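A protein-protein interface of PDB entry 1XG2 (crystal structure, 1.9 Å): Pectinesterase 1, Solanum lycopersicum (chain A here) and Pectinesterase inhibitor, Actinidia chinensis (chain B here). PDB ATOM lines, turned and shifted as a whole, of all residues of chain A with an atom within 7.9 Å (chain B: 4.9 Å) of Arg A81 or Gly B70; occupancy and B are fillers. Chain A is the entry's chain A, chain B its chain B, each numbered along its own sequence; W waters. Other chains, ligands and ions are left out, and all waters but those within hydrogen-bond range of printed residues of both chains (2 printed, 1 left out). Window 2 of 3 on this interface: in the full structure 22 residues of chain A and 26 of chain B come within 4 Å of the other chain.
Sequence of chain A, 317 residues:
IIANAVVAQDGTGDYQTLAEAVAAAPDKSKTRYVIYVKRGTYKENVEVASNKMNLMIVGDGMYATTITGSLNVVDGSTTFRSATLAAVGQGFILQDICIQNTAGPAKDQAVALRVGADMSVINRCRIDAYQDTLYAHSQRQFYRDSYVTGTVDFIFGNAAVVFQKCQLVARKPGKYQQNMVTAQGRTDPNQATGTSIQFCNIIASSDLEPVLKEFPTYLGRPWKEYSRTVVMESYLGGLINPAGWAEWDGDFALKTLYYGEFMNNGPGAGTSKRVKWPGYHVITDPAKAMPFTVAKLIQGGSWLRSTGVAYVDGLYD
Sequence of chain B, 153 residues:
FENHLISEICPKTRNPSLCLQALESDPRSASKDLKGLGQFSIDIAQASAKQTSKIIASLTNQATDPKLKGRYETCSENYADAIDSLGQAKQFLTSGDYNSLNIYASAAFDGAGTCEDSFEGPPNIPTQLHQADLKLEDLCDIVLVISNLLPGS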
ATOM      1  N   ASN A  45       2.569  27.522  -1.577  1.00  0.00           N
ATOM      2  CA  ASN A  45       1.417  27.033  -2.314  1.00  0.00           C
ATOM      3  C   ASN A  45       0.544  28.224  -2.646  1.00  0.00           C
ATOM      4  O   ASN A  45      -0.019  28.861  -1.752  1.00  0.00           O
ATOM      5  CB  ASN A  45       0.645  25.993  -1.503  1.00  0.00           C
ATOM      6  CG  ASN A  45       1.354  24.649  -1.464  1.00  0.00           C
ATOM      7  OD1 ASN A  45       2.185  24.397  -0.583  1.00  0.00           O
ATOM      8  ND2 ASN A  45       1.025  23.775  -2.409  1.00  0.00           N
ATOM      9  N   GLU A  47      -2.497  30.219  -4.969  1.00  0.00           N
ATOM     10  CA  GLU A  47      -3.784  30.051  -5.612  1.00  0.00           C
ATOM     11  C   GLU A  47      -4.154  31.338  -6.332  1.00  0.00           C
ATOM     12  O   GLU A  47      -4.052  32.418  -5.755  1.00  0.00           O
ATOM     13  CB  GLU A  47      -4.836  29.690  -4.568  1.00  0.00           C
ATOM     14  CG  GLU A  47      -6.212  29.426  -5.141  1.00  0.00           C
ATOM     15  CD  GLU A  47      -7.132  28.639  -4.203  1.00  0.00           C
ATOM     16  OE1 GLU A  47      -8.316  28.458  -4.585  1.00  0.00           O
ATOM     17  OE2 GLU A  47      -6.674  28.180  -3.113  1.00  0.00           O
ATOM     18  N   LEU A  71       2.881  19.011  -1.183  1.00  0.00           N
ATOM     19  CA  LEU A  71       1.610  18.405  -0.761  1.00  0.00           C
ATOM     20  C   LEU A  71       1.283  17.204  -1.639  1.00  0.00           C
ATOM     21  O   LEU A  71       1.635  17.162  -2.814  1.00  0.00           O
ATOM     22  CB  LEU A  71       0.457  19.414  -0.773  1.00  0.00           C
ATOM     23  CG  LEU A  71       0.696  20.712  -0.019  1.00  0.00           C
ATOM     24  CD1 LEU A  71      -0.473  21.653  -0.259  1.00  0.00           C
ATOM     25  CD2 LEU A  71       0.927  20.473   1.483  1.00  0.00           C
ATOM     26  N   ASN A  72       0.605  16.222  -1.052  1.00  0.00           N
ATOM     27  CA  ASN A  72       0.445  14.928  -1.684  1.00  0.00           C
ATOM     28  C   ASN A  72      -0.642  14.109  -1.016  1.00  0.00           C
ATOM     29  O   ASN A  72      -1.035  14.375   0.123  1.00  0.00           O
ATOM     30  CB  ASN A  72       1.768  14.158  -1.676  1.00  0.00           C
ATOM     31  CG  ASN A  72       2.260  13.842  -0.264  1.00  0.00           C
ATOM     32  OD1 ASN A  72       1.857  12.841   0.323  1.00  0.00           O
ATOM     33  ND2 ASN A  72       3.130  14.691   0.274  1.00  0.00           N
ATOM     34  N   VAL A  73      -1.103  13.095  -1.727  1.00  0.00           N
ATOM     35  CA  VAL A  73      -2.235  12.288  -1.291  1.00  0.00           C
ATOM     36  C   VAL A  73      -1.860  11.395  -0.111  1.00  0.00           C
ATOM     37  O   VAL A  73      -2.670  11.189   0.794  1.00  0.00           O
ATOM     38  CB  VAL A  73      -2.816  11.463  -2.490  1.00  0.00           C
ATOM     39  CG1 VAL A  73      -3.656  10.271  -2.037  1.00  0.00           C
ATOM     40  CG2 VAL A  73      -3.660  12.381  -3.380  1.00  0.00           C
ATOM     41  N   GLY A  76      -2.244  13.182   3.121  1.00  0.00           N
ATOM     42  CA  GLY A  76      -3.605  13.554   3.444  1.00  0.00           C
ATOM     43  C   GLY A  76      -4.232  14.668   2.628  1.00  0.00           C
ATOM     44  O   GLY A  76      -5.370  15.055   2.913  1.00  0.00           O
ATOM     45  N   SER A  77      -3.521  15.191   1.622  1.00  0.00           N
ATOM     46  CA  SER A  77      -4.142  16.129   0.694  1.00  0.00           C
ATOM     47  C   SER A  77      -5.013  15.393  -0.315  1.00  0.00           C
ATOM     48  O   SER A  77      -4.748  14.243  -0.638  1.00  0.00           O
ATOM     49  CB  SER A  77      -3.092  16.939  -0.072  1.00  0.00           C
ATOM     50  OG  SER A  77      -3.724  17.881  -0.922  1.00  0.00           O
ATOM     51  N   THR A  78      -6.046  16.055  -0.825  1.00  0.00           N
ATOM     52  CA  THR A  78      -6.664  15.594  -2.060  1.00  0.00           C
ATOM     53  C   THR A  78      -5.727  15.961  -3.204  1.00  0.00           C
ATOM     54  O   THR A  78      -4.894  16.874  -3.087  1.00  0.00           O
ATOM     55  CB  THR A  78      -8.031  16.229  -2.328  1.00  0.00           C
ATOM     56  OG1 THR A  78      -7.878  17.634  -2.542  1.00  0.00           O
ATOM     57  CG2 THR A  78      -8.961  16.110  -1.123  1.00  0.00           C
ATOM     58  N   THR A  79      -5.868  15.238  -4.300  1.00  0.00           N
ATOM     59  CA  THR A  79      -5.168  15.547  -5.529  1.00  0.00           C
ATOM     60  C   THR A  79      -5.410  16.997  -5.924  1.00  0.00           C
ATOM     61  O   THR A  79      -4.473  17.726  -6.199  1.00  0.00           O
ATOM     62  CB  THR A  79      -5.643  14.579  -6.640  1.00  0.00           C
ATOM     63  OG1 THR A  79      -5.379  13.217  -6.242  1.00  0.00           O
ATOM     64  CG2 THR A  79      -4.837  14.775  -7.921  1.00  0.00           C
ATOM     65  N   PHE A  80      -6.675  17.413  -5.915  1.00  0.00           N
ATOM     66  CA  PHE A  80      -7.075  18.749  -6.335  1.00  0.00           C
ATOM     67  C   PHE A  80      -6.352  19.829  -5.532  1.00  0.00           C
ATOM     68  O   PHE A  80      -5.887  20.805  -6.095  1.00  0.00           O
ATOM     69  CB  PHE A  80      -8.611  18.881  -6.217  1.00  0.00           C
ATOM     70  CG  PHE A  80      -9.169  20.201  -6.686  1.00  0.00           C
ATOM     71  CD1 PHE A  80      -9.423  21.222  -5.788  1.00  0.00           C
ATOM     72  CD2 PHE A  80      -9.502  20.393  -8.018  1.00  0.00           C
ATOM     73  CE1 PHE A  80      -9.970  22.434  -6.218  1.00  0.00           C
ATOM     74  CE2 PHE A  80     -10.048  21.594  -8.459  1.00  0.00           C
ATOM     75  CZ  PHE A  80     -10.283  22.620  -7.559  1.00  0.00           C
ATOM     76  N   ARG A  81      -6.240  19.636  -4.220  1.00  0.00           N
ATOM     77  CA  ARG A  81      -5.638  20.638  -3.329  1.00  0.00           C
ATOM     78  C   ARG A  81      -4.128  20.425  -3.081  1.00  0.00           C
ATOM     79  O   ARG A  81      -3.539  21.135  -2.263  1.00  0.00           O
ATOM     80  CB  ARG A  81      -6.383  20.672  -1.985  1.00  0.00           C
ATOM     81  CG  ARG A  81      -7.706  21.383  -2.008  1.00  0.00           C
ATOM     82  CD  ARG A  81      -8.362  21.460  -0.623  1.00  0.00           C
ATOM     83  NE  ARG A  81      -7.735  22.511   0.192  1.00  0.00           N
ATOM     84  CZ  ARG A  81      -7.738  22.568   1.529  1.00  0.00           C
ATOM     85  NH1 ARG A  81      -8.347  21.638   2.265  1.00  0.00           N
ATOM     86  NH2 ARG A  81      -7.116  23.575   2.140  1.00  0.00           N
ATOM     87  N   SER A  82      -3.522  19.463  -3.773  1.00  0.00           N
ATOM     88  CA  SER A  82      -2.088  19.178  -3.655  1.00  0.00           C
ATOM     89  C   SER A  82      -1.202  20.108  -4.502  1.00  0.00           C
ATOM     90  O   SER A  82       0.014  20.148  -4.312  1.00  0.00           O
ATOM     91  CB  SER A  82      -1.776  17.713  -4.023  1.00  0.00           C
ATOM     92  OG  SER A  82      -1.868  17.454  -5.429  1.00  0.00           O
ATOM     93  N   ALA A  83      -1.811  20.861  -5.417  1.00  0.00           N
ATOM     94  CA  ALA A  83      -1.061  21.706  -6.357  1.00  0.00           C
ATOM     95  C   ALA A  83      -0.167  22.739  -5.664  1.00  0.00           C
ATOM     96  O   ALA A  83      -0.612  23.471  -4.798  1.00  0.00           O
ATOM     97  CB  ALA A  83      -2.023  22.415  -7.287  1.00  0.00           C
ATOM     98  N   THR A  84       1.091  22.808  -6.077  1.00  0.00           N
ATOM     99  CA  THR A  84       1.967  23.905  -5.683  1.00  0.00           C
ATOM    100  C   THR A  84       1.386  25.242  -6.114  1.00  0.00           C
ATOM    101  O   THR A  84       1.287  26.167  -5.303  1.00  0.00           O
ATOM    102  CB  THR A  84       3.365  23.681  -6.282  1.00  0.00           C
ATOM    103  OG1 THR A  84       3.953  22.541  -5.647  1.00  0.00           O
ATOM    104  CG2 THR A  84       4.303  24.832  -5.986  1.00  0.00           C
ATOM    105  N   ALA A  86      -2.139  26.701  -8.246  1.00  0.00           N
ATOM    106  CA  ALA A  86      -3.466  26.409  -8.800  1.00  0.00           C
ATOM    107  C   ALA A  86      -4.044  27.720  -9.328  1.00  0.00           C
ATOM    108  O   ALA A  86      -3.990  28.730  -8.640  1.00  0.00           O
ATOM    109  CB  ALA A  86      -4.372  25.842  -7.728  1.00  0.00           C
ATOM    110  N   ASN A 101       6.515  20.085  -7.703  1.00  0.00           N
ATOM    111  CA  ASN A 101       6.115  19.374  -6.498  1.00  0.00           C
ATOM    112  C   ASN A 101       7.178  18.308  -6.217  1.00  0.00           C
ATOM    113  O   ASN A 101       7.418  17.421  -7.035  1.00  0.00           O
ATOM    114  CB  ASN A 101       4.713  18.787  -6.645  1.00  0.00           C
ATOM    115  CG  ASN A 101       4.177  18.232  -5.336  1.00  0.00           C
ATOM    116  OD1 ASN A 101       4.910  17.559  -4.596  1.00  0.00           O
ATOM    117  ND2 ASN A 101       2.930  18.530  -5.024  1.00  0.00           N
ATOM    118  N   VAL A 111       0.501  17.107  -7.260  1.00  0.00           N
ATOM    119  CA  VAL A 111       0.386  17.990  -8.419  1.00  0.00           C
ATOM    120  C   VAL A 111       1.340  19.169  -8.297  1.00  0.00           C
ATOM    121  O   VAL A 111       1.446  19.786  -7.226  1.00  0.00           O
ATOM    122  CB  VAL A 111      -1.072  18.513  -8.555  1.00  0.00           C
ATOM    123  CG1 VAL A 111      -1.193  19.562  -9.717  1.00  0.00           C
ATOM    124  CG2 VAL A 111      -2.039  17.368  -8.752  1.00  0.00           C
ATOM    125  N   ARG A 114      -2.019  23.018 -11.170  1.00  0.00           N
ATOM    126  CA  ARG A 114      -3.408  22.805 -11.564  1.00  0.00           C
ATOM    127  C   ARG A 114      -3.946  24.049 -12.248  1.00  0.00           C
ATOM    128  O   ARG A 114      -3.842  25.157 -11.731  1.00  0.00           O
ATOM    129  CB  ARG A 114      -4.297  22.440 -10.385  1.00  0.00           C
ATOM    130  CG  ARG A 114      -5.786  22.486 -10.711  1.00  0.00           C
ATOM    131  CD  ARG A 114      -6.651  21.788  -9.684  1.00  0.00           C
ATOM    132  NE  ARG A 114      -6.533  22.404  -8.365  1.00  0.00           N
ATOM    133  CZ  ARG A 114      -7.100  23.559  -8.004  1.00  0.00           C
ATOM    134  NH1 ARG A 114      -7.851  24.254  -8.848  1.00  0.00           N
ATOM    135  NH2 ARG A 114      -6.920  24.018  -6.769  1.00  0.00           N
ATOM    136  N   TYR A 135      -2.283  18.963 -13.658  1.00  0.00           N
ATOM    137  CA  TYR A 135      -3.728  18.820 -13.597  1.00  0.00           C
ATOM    138  C   TYR A 135      -4.365  19.898 -14.464  1.00  0.00           C
ATOM    139  O   TYR A 135      -4.702  20.986 -13.978  1.00  0.00           O
ATOM    140  CB  TYR A 135      -4.187  18.973 -12.132  1.00  0.00           C
ATOM    141  CG  TYR A 135      -5.520  18.362 -11.754  1.00  0.00           C
ATOM    142  CD1 TYR A 135      -6.430  17.920 -12.702  1.00  0.00           C
ATOM    143  CD2 TYR A 135      -5.846  18.201 -10.406  1.00  0.00           C
ATOM    144  CE1 TYR A 135      -7.642  17.347 -12.324  1.00  0.00           C
ATOM    145  CE2 TYR A 135      -7.036  17.636 -10.019  1.00  0.00           C
ATOM    146  CZ  TYR A 135      -7.934  17.210 -10.965  1.00  0.00           C
ATOM    147  OH  TYR A 135      -9.114  16.650 -10.533  1.00  0.00           O
ATOM    148  N   PRO B  66      -9.422  15.666  10.098  1.00  0.00           N
ATOM    149  CA  PRO B  66      -8.744  16.513   9.101  1.00  0.00           C
ATOM    150  C   PRO B  66      -8.809  16.029   7.639  1.00  0.00           C
ATOM    151  O   PRO B  66      -8.942  16.864   6.741  1.00  0.00           O
ATOM    152  CB  PRO B  66      -7.291  16.535   9.592  1.00  0.00           C
ATOM    153  CG  PRO B  66      -7.410  16.354  11.066  1.00  0.00           C
ATOM    154  CD  PRO B  66      -8.510  15.321  11.207  1.00  0.00           C
ATOM    155  N   LYS B  67      -8.726  14.724   7.407  1.00  0.00           N
ATOM    156  CA  LYS B  67      -8.749  14.202   6.040  1.00  0.00           C
ATOM    157  C   LYS B  67     -10.122  14.413   5.415  1.00  0.00           C
ATOM    158  O   LYS B  67     -10.237  14.852   4.271  1.00  0.00           O
ATOM    159  CB  LYS B  67      -8.378  12.721   6.006  1.00  0.00           C
ATOM    160  CG  LYS B  67      -8.063  12.186   4.601  1.00  0.00           C
ATOM    161  CD  LYS B  67      -7.550  10.748   4.665  1.00  0.00           C
ATOM    162  CE  LYS B  67      -7.558  10.069   3.308  1.00  0.00           C
ATOM    163  NZ  LYS B  67      -6.588   8.927   3.223  1.00  0.00           N
ATOM    164  N   LEU B  68     -11.160  14.105   6.186  1.00  0.00           N
ATOM    165  CA  LEU B  68     -12.529  14.285   5.739  1.00  0.00           C
ATOM    166  C   LEU B  68     -12.809  15.755   5.452  1.00  0.00           C
ATOM    167  O   LEU B  68     -13.415  16.080   4.435  1.00  0.00           O
ATOM    168  CB  LEU B  68     -13.512  13.746   6.788  1.00  0.00           C
ATOM    169  CG  LEU B  68     -15.001  13.896   6.467  1.00  0.00           C
ATOM    170  CD1 LEU B  68     -15.406  13.142   5.183  1.00  0.00           C
ATOM    171  CD2 LEU B  68     -15.828  13.420   7.657  1.00  0.00           C
ATOM    172  N   LYS B  69     -12.363  16.633   6.349  1.00  0.00           N
ATOM    173  CA  LYS B  69     -12.555  18.067   6.185  1.00  0.00           C
ATOM    174  C   LYS B  69     -11.867  18.575   4.916  1.00  0.00           C
ATOM    175  O   LYS B  69     -12.380  19.464   4.246  1.00  0.00           O
ATOM    176  CB  LYS B  69     -12.023  18.826   7.392  1.00  0.00           C
ATOM    177  CG  LYS B  69     -12.832  18.579   8.659  1.00  0.00           C
ATOM    178  CD  LYS B  69     -12.451  19.547   9.769  1.00  0.00           C
ATOM    179  CE  LYS B  69     -13.127  20.900   9.579  1.00  0.00           C
ATOM    180  NZ  LYS B  69     -12.251  22.014  10.055  1.00  0.00           N
ATOM    181  N   GLY B  70     -10.705  18.012   4.608  1.00  0.00           N
ATOM    182  CA  GLY B  70      -9.984  18.367   3.389  1.00  0.00           C
ATOM    183  C   GLY B  70     -10.742  17.935   2.136  1.00  0.00           C
ATOM    184  O   GLY B  70     -10.687  18.613   1.120  1.00  0.00           O
ATOM    185  N   ARG B  71     -11.428  16.799   2.207  1.00  0.00           N
ATOM    186  CA  ARG B  71     -12.282  16.339   1.114  1.00  0.00           C
ATOM    187  C   ARG B  71     -13.474  17.274   0.919  1.00  0.00           C
ATOM    188  O   ARG B  71     -13.777  17.701  -0.215  1.00  0.00           O
ATOM    189  CB  ARG B  71     -12.717  14.892   1.328  1.00  0.00           C
ATOM    190  CG  ARG B  71     -11.560  13.936   1.218  1.00  0.00           C
ATOM    191  CD  ARG B  71     -11.886  12.502   1.570  1.00  0.00           C
ATOM    192  NE  ARG B  71     -10.771  11.646   1.208  1.00  0.00           N
ATOM    193  CZ  ARG B  71     -10.860  10.361   0.914  1.00  0.00           C
ATOM    194  NH1 ARG B  71      -9.767   9.703   0.562  1.00  0.00           N
ATOM    195  NH2 ARG B  71     -12.013   9.717   0.995  1.00  0.00           N
ATOM    196  N   TYR B  72     -14.125  17.652   2.017  1.00  0.00           N
ATOM    197  CA  TYR B  72     -15.225  18.600   1.931  1.00  0.00           C
ATOM    198  C   TYR B  72     -14.765  19.960   1.416  1.00  0.00           C
ATOM    199  O   TYR B  72     -15.496  20.627   0.694  1.00  0.00           O
ATOM    200  CB  TYR B  72     -15.890  18.803   3.285  1.00  0.00           C
ATOM    201  CG  TYR B  72     -16.666  17.621   3.828  1.00  0.00           C
ATOM    202  CD1 TYR B  72     -16.747  17.403   5.207  1.00  0.00           C
ATOM    203  CD2 TYR B  72     -17.352  16.741   2.980  1.00  0.00           C
ATOM    204  CE1 TYR B  72     -17.468  16.338   5.728  1.00  0.00           C
ATOM    205  CE2 TYR B  72     -18.063  15.671   3.486  1.00  0.00           C
ATOM    206  CZ  TYR B  72     -18.130  15.474   4.865  1.00  0.00           C
ATOM    207  OH  TYR B  72     -18.851  14.406   5.368  1.00  0.00           O
ATOM    208  N   GLU B  73     -13.564  20.385   1.798  1.00  0.00           N
ATOM    209  CA  GLU B  73     -13.096  21.699   1.375  1.00  0.00           C
ATOM    210  C   GLU B  73     -12.839  21.688  -0.126  1.00  0.00           C
ATOM    211  O   GLU B  73     -13.126  22.658  -0.811  1.00  0.00           O
ATOM    212  CB  GLU B  73     -11.856  22.150   2.141  1.00  0.00           C
ATOM    213  CG  GLU B  73     -11.424  23.581   1.797  1.00  0.00           C
ATOM    214  CD  GLU B  73     -12.502  24.645   2.082  1.00  0.00           C
ATOM    215  OE1 GLU B  73     -13.240  24.514   3.091  1.00  0.00           O
ATOM    216  OE2 GLU B  73     -12.622  25.628   1.296  1.00  0.00           O
ATOM    217  N   THR B  74     -12.333  20.573  -0.631  1.00  0.00           N
ATOM    218  CA  THR B  74     -12.116  20.403  -2.068  1.00  0.00           C
ATOM    219  C   THR B  74     -13.469  20.458  -2.792  1.00  0.00           C
ATOM    220  O   THR B  74     -13.631  21.147  -3.804  1.00  0.00           O
ATOM    221  CB  THR B  74     -11.397  19.064  -2.305  1.00  0.00           C
ATOM    222  OG1 THR B  74     -10.032  19.171  -1.881  1.00  0.00           O
ATOM    223  CG2 THR B  74     -11.310  18.705  -3.780  1.00  0.00           C
ATOM    224  N   GLU B  77     -14.703  24.061  -2.899  1.00  0.00           N
ATOM    225  CA  GLU B  77     -14.004  24.882  -3.907  1.00  0.00           C
ATOM    226  C   GLU B  77     -14.500  24.573  -5.322  1.00  0.00           C
ATOM    227  O   GLU B  77     -14.726  25.475  -6.126  1.00  0.00           O
ATOM    228  CB  GLU B  77     -12.492  24.675  -3.803  1.00  0.00           C
ATOM    229  CG  GLU B  77     -11.905  25.296  -2.542  1.00  0.00           C
ATOM    230  CD  GLU B  77     -10.436  24.942  -2.285  1.00  0.00           C
ATOM    231  OE1 GLU B  77      -9.931  25.299  -1.187  1.00  0.00           O
ATOM    232  OE2 GLU B  77      -9.790  24.318  -3.151  1.00  0.00           O
HETATM  233  O   HOH W   1      -3.649  10.378   4.360  1.00  0.00           O
HETATM  234  O   HOH W   2      -8.344  15.205   2.462  1.00  0.00           O
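The side-chain hydroxyl of Thr A78 sits at hydrogen-bond distance from the side-chain hydroxyl of Thr B74, 2.7 Å away.
NE of Arg A81 is in salt-bridge range of OE1 of Glu B77.
Of the 19 printed residues of chain A, 3 touch a printed residue of chain B.
Hydrophobic or aromatic side chains of chain A within 4 Å of the printed part of chain B: Phe A80.
Of the 10 printed residues of chain B, 4 touch a printed residue of chain A.
Among the printed residues, 8 pairs touch across the chains.
Among the printed residues, Asp or Glu carboxylates within 4 Å of a Lys or Arg side-chain nitrogen of the other chain: Arg A81 with Glu B77 (3.8 Å).
Among the printed residues, pairs that only touch across the chains: Thr A78 with Gly B70, Phe A80 with Thr B74, Phe A80 with Glu B77, Arg A81 with Gly B70, Arg A81 with Glu B73 and Arg A81 with Thr B74.
Water W2 lies within hydrogen-bond range of the backbone carbonyl oxygen (O) of Lys B67, the backbone carbonyl oxygen (O) of Gly A76 and the backbone NH (N) of Arg B71.
Water W1 lies within hydrogen-bond range of N of Gly A76 (3.4 Å) and NZ of Lys B67 (3.5 Å).
Of the printed residues of chain B, Thr A78 touches Gly B70 and Thr B74.
Printed residues of chain B within 4 Å of Phe A80: Thr B74 and Glu B77.
Arg A81 touches just these residues of chain B: Gly B70 (3.8 Å), Glu B73 (3.5 Å), Thr B74 (3.1 Å) and Glu B77 (3.8 Å).
Leu B68 touches none of the printed residues of chain A.
Gly B70 touches two residues of chain A.
Of the printed residues of chain A, Glu B77 touches Phe A80 and Arg A81.
The nearest printed residue of chain B that does not touch Arg A81 is Lys B69 (5.0 Å).
The nearest printed residue of chain B that does not touch Thr A78 is Arg B71 (4.01 Å).
N of Arg A81 sits at hydrogen-bond distance from OG1 of Thr A78 (3.1 Å).
The backbone carbonyl oxygen of Phe A80 is in hydrogen-bond range of the guanidinium group of Arg A114 (2.9 Å).
The backbone carbonyl oxygen of Gly B70 lies within hydrogen-bond range of the side-chain hydroxyl of Thr B74 (3.1 Å).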
